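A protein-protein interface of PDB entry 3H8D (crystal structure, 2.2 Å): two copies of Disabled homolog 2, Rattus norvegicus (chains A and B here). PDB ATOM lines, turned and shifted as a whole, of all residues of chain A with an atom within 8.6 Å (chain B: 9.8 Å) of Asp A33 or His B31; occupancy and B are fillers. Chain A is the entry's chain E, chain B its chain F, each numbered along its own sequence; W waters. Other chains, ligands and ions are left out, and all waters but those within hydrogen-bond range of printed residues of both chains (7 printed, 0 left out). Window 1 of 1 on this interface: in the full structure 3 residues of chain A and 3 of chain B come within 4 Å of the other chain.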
ATOM      1  N   GLU A  30      10.068   0.694   6.295  1.00  0.00           N
ATOM      2  CA  GLU A  30      11.153   1.529   5.796  1.00  0.00           C
ATOM      3  C   GLU A  30      12.465   1.227   6.528  1.00  0.00           C
ATOM      4  O   GLU A  30      12.467   0.909   7.718  1.00  0.00           O
ATOM      5  CB  GLU A  30      10.771   3.009   5.953  1.00  0.00           C
ATOM      6  CG  GLU A  30      11.199   3.924   4.805  1.00  0.00           C
ATOM      7  CD  GLU A  30      10.684   3.481   3.426  1.00  0.00           C
ATOM      8  OE1 GLU A  30       9.487   3.148   3.282  1.00  0.00           O
ATOM      9  OE2 GLU A  30      11.490   3.484   2.473  1.00  0.00           O
ATOM     10  N   HIS A  31      13.575   1.285   5.804  1.00  0.00           N
ATOM     11  CA  HIS A  31      14.875   1.279   6.452  1.00  0.00           C
ATOM     12  C   HIS A  31      15.324   2.714   6.705  1.00  0.00           C
ATOM     13  O   HIS A  31      15.364   3.525   5.788  1.00  0.00           O
ATOM     14  CB  HIS A  31      15.928   0.531   5.632  1.00  0.00           C
ATOM     15  CG  HIS A  31      17.322   0.744   6.131  1.00  0.00           C
ATOM     16  ND1 HIS A  31      17.784   0.183   7.301  1.00  0.00           N
ATOM     17  CD2 HIS A  31      18.335   1.504   5.654  1.00  0.00           C
ATOM     18  CE1 HIS A  31      19.036   0.556   7.502  1.00  0.00           C
ATOM     19  NE2 HIS A  31      19.389   1.366   6.522  1.00  0.00           N
ATOM     20  N   VAL A  32      15.681   3.010   7.951  1.00  0.00           N
ATOM     21  CA  VAL A  32      16.127   4.352   8.325  1.00  0.00           C
ATOM     22  C   VAL A  32      17.655   4.457   8.417  1.00  0.00           C
ATOM     23  O   VAL A  32      18.298   3.759   9.207  1.00  0.00           O
ATOM     24  CB  VAL A  32      15.469   4.832   9.654  1.00  0.00           C
ATOM     25  CG1 VAL A  32      15.888   6.252   9.967  1.00  0.00           C
ATOM     26  CG2 VAL A  32      13.931   4.724   9.582  1.00  0.00           C
ATOM     27  N   ASP A  33      18.225   5.317   7.583  1.00  0.00           N
ATOM     28  CA  ASP A  33      19.603   5.766   7.749  1.00  0.00           C
ATOM     29  C   ASP A  33      19.596   7.279   7.993  1.00  0.00           C
ATOM     30  O   ASP A  33      19.448   8.046   7.050  1.00  0.00           O
ATOM     31  CB  ASP A  33      20.461   5.401   6.514  1.00  0.00           C
ATOM     32  CG  ASP A  33      21.960   5.535   6.776  1.00  0.00           C
ATOM     33  OD1 ASP A  33      22.381   6.468   7.485  1.00  0.00           O
ATOM     34  OD2 ASP A  33      22.733   4.693   6.296  1.00  0.00           O
ATOM     35  N   HIS A  34      19.738   7.687   9.256  1.00  0.00           N
ATOM     36  CA  HIS A  34      19.808   9.110   9.646  1.00  0.00           C
ATOM     37  C   HIS A  34      21.014   9.817   9.049  1.00  0.00           C
ATOM     38  O   HIS A  34      20.998  11.030   8.877  1.00  0.00           O
ATOM     39  CB  HIS A  34      19.884   9.280  11.168  1.00  0.00           C
ATOM     40  CG  HIS A  34      18.675   8.786  11.905  1.00  0.00           C
ATOM     41  ND1 HIS A  34      17.432   9.371  11.782  1.00  0.00           N
ATOM     42  CD2 HIS A  34      18.526   7.771  12.790  1.00  0.00           C
ATOM     43  CE1 HIS A  34      16.566   8.731  12.547  1.00  0.00           C
ATOM     44  NE2 HIS A  34      17.205   7.756  13.171  1.00  0.00           N
ATOM     45  N   ASP A  35      22.071   9.067   8.756  1.00  0.00           N
ATOM     46  CA  ASP A  35      23.280   9.689   8.230  1.00  0.00           C
ATOM     47  C   ASP A  35      23.152  10.056   6.749  1.00  0.00           C
ATOM     48  O   ASP A  35      23.717  11.062   6.313  1.00  0.00           O
ATOM     49  CB  ASP A  35      24.508   8.844   8.540  1.00  0.00           C
ATOM     50  CG  ASP A  35      24.855   8.864  10.011  1.00  0.00           C
ATOM     51  OD1 ASP A  35      24.947   9.978  10.573  1.00  0.00           O
ATOM     52  OD2 ASP A  35      25.029   7.781  10.611  1.00  0.00           O
ATOM     53  N   ASP A  36      22.376   9.260   6.005  1.00  0.00           N
ATOM     54  CA  ASP A  36      21.994   9.572   4.622  1.00  0.00           C
ATOM     55  C   ASP A  36      21.019  10.745   4.611  1.00  0.00           C
ATOM     56  O   ASP A  36      21.162  11.687   3.830  1.00  0.00           O
ATOM     57  CB  ASP A  36      21.298   8.373   3.959  1.00  0.00           C
ATOM     58  CG  ASP A  36      22.255   7.247   3.578  1.00  0.00           C
ATOM     59  OD1 ASP A  36      23.492   7.386   3.693  1.00  0.00           O
ATOM     60  OD2 ASP A  36      21.755   6.206   3.126  1.00  0.00           O
ATOM     61  N   PHE A  37      20.011  10.650   5.477  1.00  0.00           N
ATOM     62  CA  PHE A  37      18.945  11.622   5.565  1.00  0.00           C
ATOM     63  C   PHE A  37      19.465  12.993   5.994  1.00  0.00           C
ATOM     64  O   PHE A  37      19.220  13.995   5.309  1.00  0.00           O
ATOM     65  CB  PHE A  37      17.854  11.148   6.544  1.00  0.00           C
ATOM     66  CG  PHE A  37      16.657  12.056   6.586  1.00  0.00           C
ATOM     67  CD1 PHE A  37      15.676  11.975   5.601  1.00  0.00           C
ATOM     68  CD2 PHE A  37      16.524  13.009   7.591  1.00  0.00           C
ATOM     69  CE1 PHE A  37      14.574  12.822   5.624  1.00  0.00           C
ATOM     70  CE2 PHE A  37      15.428  13.862   7.625  1.00  0.00           C
ATOM     71  CZ  PHE A  37      14.453  13.773   6.646  1.00  0.00           C
ATOM     72  N   ASP A  38      20.189  13.026   7.111  1.00  0.00           N
ATOM     73  CA  ASP A  38      20.679  14.280   7.678  1.00  0.00           C
ATOM     74  C   ASP A  38      21.710  14.964   6.779  1.00  0.00           C
ATOM     75  O   ASP A  38      21.764  16.192   6.717  1.00  0.00           O
ATOM     76  CB  ASP A  38      21.271  14.058   9.067  1.00  0.00           C
ATOM     77  CG  ASP A  38      20.244  13.590  10.087  1.00  0.00           C
ATOM     78  OD1 ASP A  38      19.030  13.720   9.834  1.00  0.00           O
ATOM     79  OD2 ASP A  38      20.670  13.086  11.154  1.00  0.00           O
ATOM     80  N   ALA A  39      22.534  14.171   6.096  1.00  0.00           N
ATOM     81  CA  ALA A  39      23.546  14.723   5.181  1.00  0.00           C
ATOM     82  C   ALA A  39      22.873  15.369   3.977  1.00  0.00           C
ATOM     83  O   ALA A  39      23.294  16.432   3.523  1.00  0.00           O
ATOM     84  CB  ALA A  39      24.522  13.641   4.740  1.00  0.00           C
ATOM     85  N   ASN A  40      21.834  14.711   3.464  1.00  0.00           N
ATOM     86  CA  ASN A  40      21.029  15.260   2.381  1.00  0.00           C
ATOM     87  C   ASN A  40      20.218  16.478   2.816  1.00  0.00           C
ATOM     88  O   ASN A  40      20.048  17.390   2.042  1.00  0.00           O
ATOM     89  CB  ASN A  40      20.127  14.184   1.768  1.00  0.00           C
ATOM     90  CG  ASN A  40      20.861  13.318   0.744  1.00  0.00           C
ATOM     91  OD1 ASN A  40      21.299  13.806  -0.302  1.00  0.00           O
ATOM     92  ND2 ASN A  40      20.980  12.027   1.037  1.00  0.00           N
ATOM     93  N   PRO B  28      34.401  11.696  16.318  1.00  0.00           N
ATOM     94  CA  PRO B  28      33.638  10.681  15.622  1.00  0.00           C
ATOM     95  C   PRO B  28      32.378  10.315  16.387  1.00  0.00           C
ATOM     96  O   PRO B  28      32.407  10.197  17.610  1.00  0.00           O
ATOM     97  CB  PRO B  28      34.598   9.493  15.567  1.00  0.00           C
ATOM     98  CG  PRO B  28      35.957  10.034  16.029  1.00  0.00           C
ATOM     99  CD  PRO B  28      35.643  11.158  16.907  1.00  0.00           C
ATOM    100  N   GLN B  29      31.276  10.174  15.657  1.00  0.00           N
ATOM    101  CA  GLN B  29      30.002   9.746  16.213  1.00  0.00           C
ATOM    102  C   GLN B  29      29.609   8.376  15.638  1.00  0.00           C
ATOM    103  O   GLN B  29      30.142   7.948  14.603  1.00  0.00           O
ATOM    104  CB  GLN B  29      28.925  10.779  15.895  1.00  0.00           C
ATOM    105  CG  GLN B  29      29.231  12.173  16.410  1.00  0.00           C
ATOM    106  CD  GLN B  29      29.055  12.299  17.926  1.00  0.00           C
ATOM    107  OE1 GLN B  29      29.935  11.930  18.706  1.00  0.00           O
ATOM    108  NE2 GLN B  29      27.916  12.831  18.338  1.00  0.00           N
ATOM    109  N   GLU B  30      28.682   7.698  16.310  1.00  0.00           N
ATOM    110  CA  GLU B  30      28.209   6.387  15.871  1.00  0.00           C
ATOM    111  C   GLU B  30      27.245   6.484  14.681  1.00  0.00           C
ATOM    112  O   GLU B  30      26.434   7.424  14.563  1.00  0.00           O
ATOM    113  CB  GLU B  30      27.544   5.609  17.029  1.00  0.00           C
ATOM    114  CG  GLU B  30      26.276   6.270  17.598  1.00  0.00           C
ATOM    115  CD  GLU B  30      25.446   5.363  18.508  1.00  0.00           C
ATOM    116  OE1 GLU B  30      25.798   4.176  18.693  1.00  0.00           O
ATOM    117  OE2 GLU B  30      24.421   5.850  19.033  1.00  0.00           O
ATOM    118  N   HIS B  31      27.355   5.503  13.795  1.00  0.00           N
ATOM    119  CA  HIS B  31      26.320   5.262  12.819  1.00  0.00           C
ATOM    120  C   HIS B  31      25.373   4.196  13.374  1.00  0.00           C
ATOM    121  O   HIS B  31      25.820   3.130  13.793  1.00  0.00           O
ATOM    122  CB  HIS B  31      26.906   4.809  11.483  1.00  0.00           C
ATOM    123  CG  HIS B  31      25.881   4.244  10.549  1.00  0.00           C
ATOM    124  ND1 HIS B  31      24.992   5.036   9.851  1.00  0.00           N
ATOM    125  CD2 HIS B  31      25.583   2.965  10.222  1.00  0.00           C
ATOM    126  CE1 HIS B  31      24.205   4.269   9.122  1.00  0.00           C
ATOM    127  NE2 HIS B  31      24.541   3.008   9.330  1.00  0.00           N
ATOM    128  N   VAL B  32      24.077   4.494  13.360  1.00  0.00           N
ATOM    129  CA  VAL B  32      23.040   3.569  13.822  1.00  0.00           C
ATOM    130  C   VAL B  32      22.365   2.823  12.657  1.00  0.00           C
ATOM    131  O   VAL B  32      21.925   3.437  11.681  1.00  0.00           O
ATOM    132  CB  VAL B  32      21.968   4.327  14.660  1.00  0.00           C
ATOM    133  CG1 VAL B  32      20.767   3.437  14.982  1.00  0.00           C
ATOM    134  CG2 VAL B  32      22.587   4.880  15.958  1.00  0.00           C
ATOM    135  N   ASP B  33      22.307   1.496  12.756  1.00  0.00           N
ATOM    136  CA  ASP B  33      21.450   0.696  11.884  1.00  0.00           C
ATOM    137  C   ASP B  33      20.537  -0.166  12.744  1.00  0.00           C
ATOM    138  O   ASP B  33      20.932  -1.245  13.191  1.00  0.00           O
ATOM    139  CB  ASP B  33      22.277  -0.166  10.914  1.00  0.00           C
ATOM    140  CG  ASP B  33      21.428  -0.808   9.811  1.00  0.00           C
ATOM    141  OD1 ASP B  33      20.265  -1.198  10.059  1.00  0.00           O
ATOM    142  OD2 ASP B  33      21.928  -0.926   8.674  1.00  0.00           O
ATOM    143  N   HIS B  34      19.316   0.325  12.973  1.00  0.00           N
ATOM    144  CA  HIS B  34      18.286  -0.409  13.724  1.00  0.00           C
ATOM    145  C   HIS B  34      17.971  -1.782  13.146  1.00  0.00           C
ATOM    146  O   HIS B  34      17.696  -2.714  13.893  1.00  0.00           O
ATOM    147  CB  HIS B  34      16.983   0.392  13.814  1.00  0.00           C
ATOM    148  CG  HIS B  34      17.093   1.654  14.611  1.00  0.00           C
ATOM    149  ND1 HIS B  34      17.542   1.678  15.913  1.00  0.00           N
ATOM    150  CD2 HIS B  34      16.790   2.936  14.292  1.00  0.00           C
ATOM    151  CE1 HIS B  34      17.526   2.921  16.360  1.00  0.00           C
ATOM    152  NE2 HIS B  34      17.072   3.704  15.396  1.00  0.00           N
ATOM    153  N   ASP B  35      18.010  -1.910  11.821  1.00  0.00           N
ATOM    154  CA  ASP B  35      17.716  -3.205  11.183  1.00  0.00           C
ATOM    155  C   ASP B  35      18.806  -4.274  11.369  1.00  0.00           C
ATOM    156  O   ASP B  35      18.484  -5.464  11.445  1.00  0.00           O
ATOM    157  CB  ASP B  35      17.311  -3.027   9.713  1.00  0.00           C
ATOM    158  CG  ASP B  35      15.996  -2.240   9.562  1.00  0.00           C
ATOM    159  OD1 ASP B  35      14.997  -2.602  10.217  1.00  0.00           O
ATOM    160  OD2 ASP B  35      15.968  -1.253   8.800  1.00  0.00           O
ATOM    161  N   ASP B  36      20.072  -3.851  11.467  1.00  0.00           N
ATOM    162  CA  ASP B  36      21.184  -4.758  11.791  1.00  0.00           C
ATOM    163  C   ASP B  36      21.069  -5.156  13.253  1.00  0.00           C
ATOM    164  O   ASP B  36      21.207  -6.325  13.602  1.00  0.00           O
ATOM    165  CB  ASP B  36      22.557  -4.087  11.602  1.00  0.00           C
ATOM    166  CG  ASP B  36      22.973  -3.936  10.140  1.00  0.00           C
ATOM    167  OD1 ASP B  36      23.759  -3.006   9.866  1.00  0.00           O
ATOM    168  OD2 ASP B  36      22.547  -4.723   9.264  1.00  0.00           O
ATOM    169  N   PHE B  37      20.836  -4.163  14.105  1.00  0.00           N
ATOM    170  CA  PHE B  37      20.717  -4.378  15.545  1.00  0.00           C
ATOM    171  C   PHE B  37      19.552  -5.306  15.912  1.00  0.00           C
ATOM    172  O   PHE B  37      19.758  -6.341  16.547  1.00  0.00           O
ATOM    173  CB  PHE B  37      20.649  -3.032  16.301  1.00  0.00           C
ATOM    174  CG  PHE B  37      20.699  -3.183  17.792  1.00  0.00           C
ATOM    175  CD1 PHE B  37      21.917  -3.232  18.456  1.00  0.00           C
ATOM    176  CD2 PHE B  37      19.524  -3.325  18.535  1.00  0.00           C
ATOM    177  CE1 PHE B  37      21.969  -3.402  19.843  1.00  0.00           C
ATOM    178  CE2 PHE B  37      19.566  -3.496  19.923  1.00  0.00           C
ATOM    179  CZ  PHE B  37      20.793  -3.531  20.578  1.00  0.00           C
HETATM  180  O   HOH W   1      20.994   2.796   9.217  1.00  0.00           O
HETATM  181  O   HOH W   2      17.959   2.074  11.017  1.00  0.00           O
HETATM  182  O   HOH W   3      23.282   7.072  12.500  1.00  0.00           O
HETATM  183  O   HOH W   4      21.155   5.946  11.153  1.00  0.00           O
HETATM  184  O   HOH W   5      25.520   9.646  13.285  1.00  0.00           O
HETATM  185  O   HOH W   6      15.370   1.222  10.157  1.00  0.00           O
HETATM  186  O   HOH W   7      12.705  -1.061   9.787  1.00  0.00           O
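Water W2 bridges the backbone carbonyl oxygen (O) of Val A32 and the backbone NH (N) of His B34.
Water W3 bridges OD2 of Asp A35 (2.7 Å) and N of Val B32 (2.8 Å).
Water W4 lies within hydrogen-bond range of O of Val B32 (2.7 Å) and N of His A34 (2.9 Å).
Water W1 lies within hydrogen-bond range of O of Val B32, O of Val A32 and NE2 of His A31.
Water W7 bridges the side-chain carboxylate (OD1) of Asp B35 (2.8 Å) and the backbone carbonyl oxygen (O) of Glu A30 (2.9 Å).
Water W6 lies within hydrogen-bond range of the backbone NH of Val A32 (2.9 Å) and the side-chain carboxylate of Asp B35 (2.9 Å).
Of the 10 printed residues of chain B, 3 touch a printed residue of chain A.
Hydrophobic or aromatic side chains of chain B within 4 Å of the printed part of chain A: His B31.
Hydrophobic or aromatic side chains of chain A within 4 Å of the printed part of chain B: His A31.
The side-chain carboxylate (OD1) of Asp A33 sits at hydrogen-bond distance from the backbone NH (N) of Asp A35 (2.9 Å).
OD1 of Asp A33 sits at hydrogen-bond distance from N of Asp A36, at 3.2 Å.
The backbone NH (N) of Asp B35 is in hydrogen-bond range of the side-chain carboxylate (OD1) of Asp B33 (2.9 Å).
The backbone NH (N) of Asp B36 lies within hydrogen-bond range of the side-chain carboxylate (OD1) of Asp B33 (3.0 Å).
His A31 touches Asp B33, and with the chains exchanged Asp A33 touches His B31.
His A31 touches Asp B35, and with the chains exchanged Asp A35 touches His B31.
Of the 4 pairs that touch across the chains among the printed residues, 4 have their exchanged pair printed and touching as well.
Glu A30 touches none of the printed residues of chain B.
Of the printed residues of chain B, His A31 touches Asp B33 (3.3 Å) and Asp B35 (2.8 Å).
Asp A33 touches just one residue of chain B: His B31 (3.2 Å).
Of chain B, only His B31 comes within 4 Å of Asp A35.
No residue of chain B comes within 4 Å of Asp A36.
His B31 touches two residues of chain A.
Of the printed residues of chain A, Asp B33 touches His A31.
Of the printed residues of chain A, Asp B35 touches His A31.
Phe B37 touches none of the printed residues of chain A.
The nearest residue of chain B that does not touch Asp A33 is Val B32 (5.1 Å).
The nearest residue of chain A that does not touch His B31 is His A34 (5.6 Å).
The side-chain carboxylate of Asp B35 is in hydrogen-bond range of a ring nitrogen (ND1) of His A31, 2.8 Å away.
The side-chain carboxylate of Asp A35 lies within hydrogen-bond range of a ring nitrogen (ND1) of His B31, at 2.8 Å.
OD1 of Asp B33 touches CE1 of His A31 (3.3 Å).
OD2 of Asp A33 touches CE1 of His B31 (3.2 Å).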
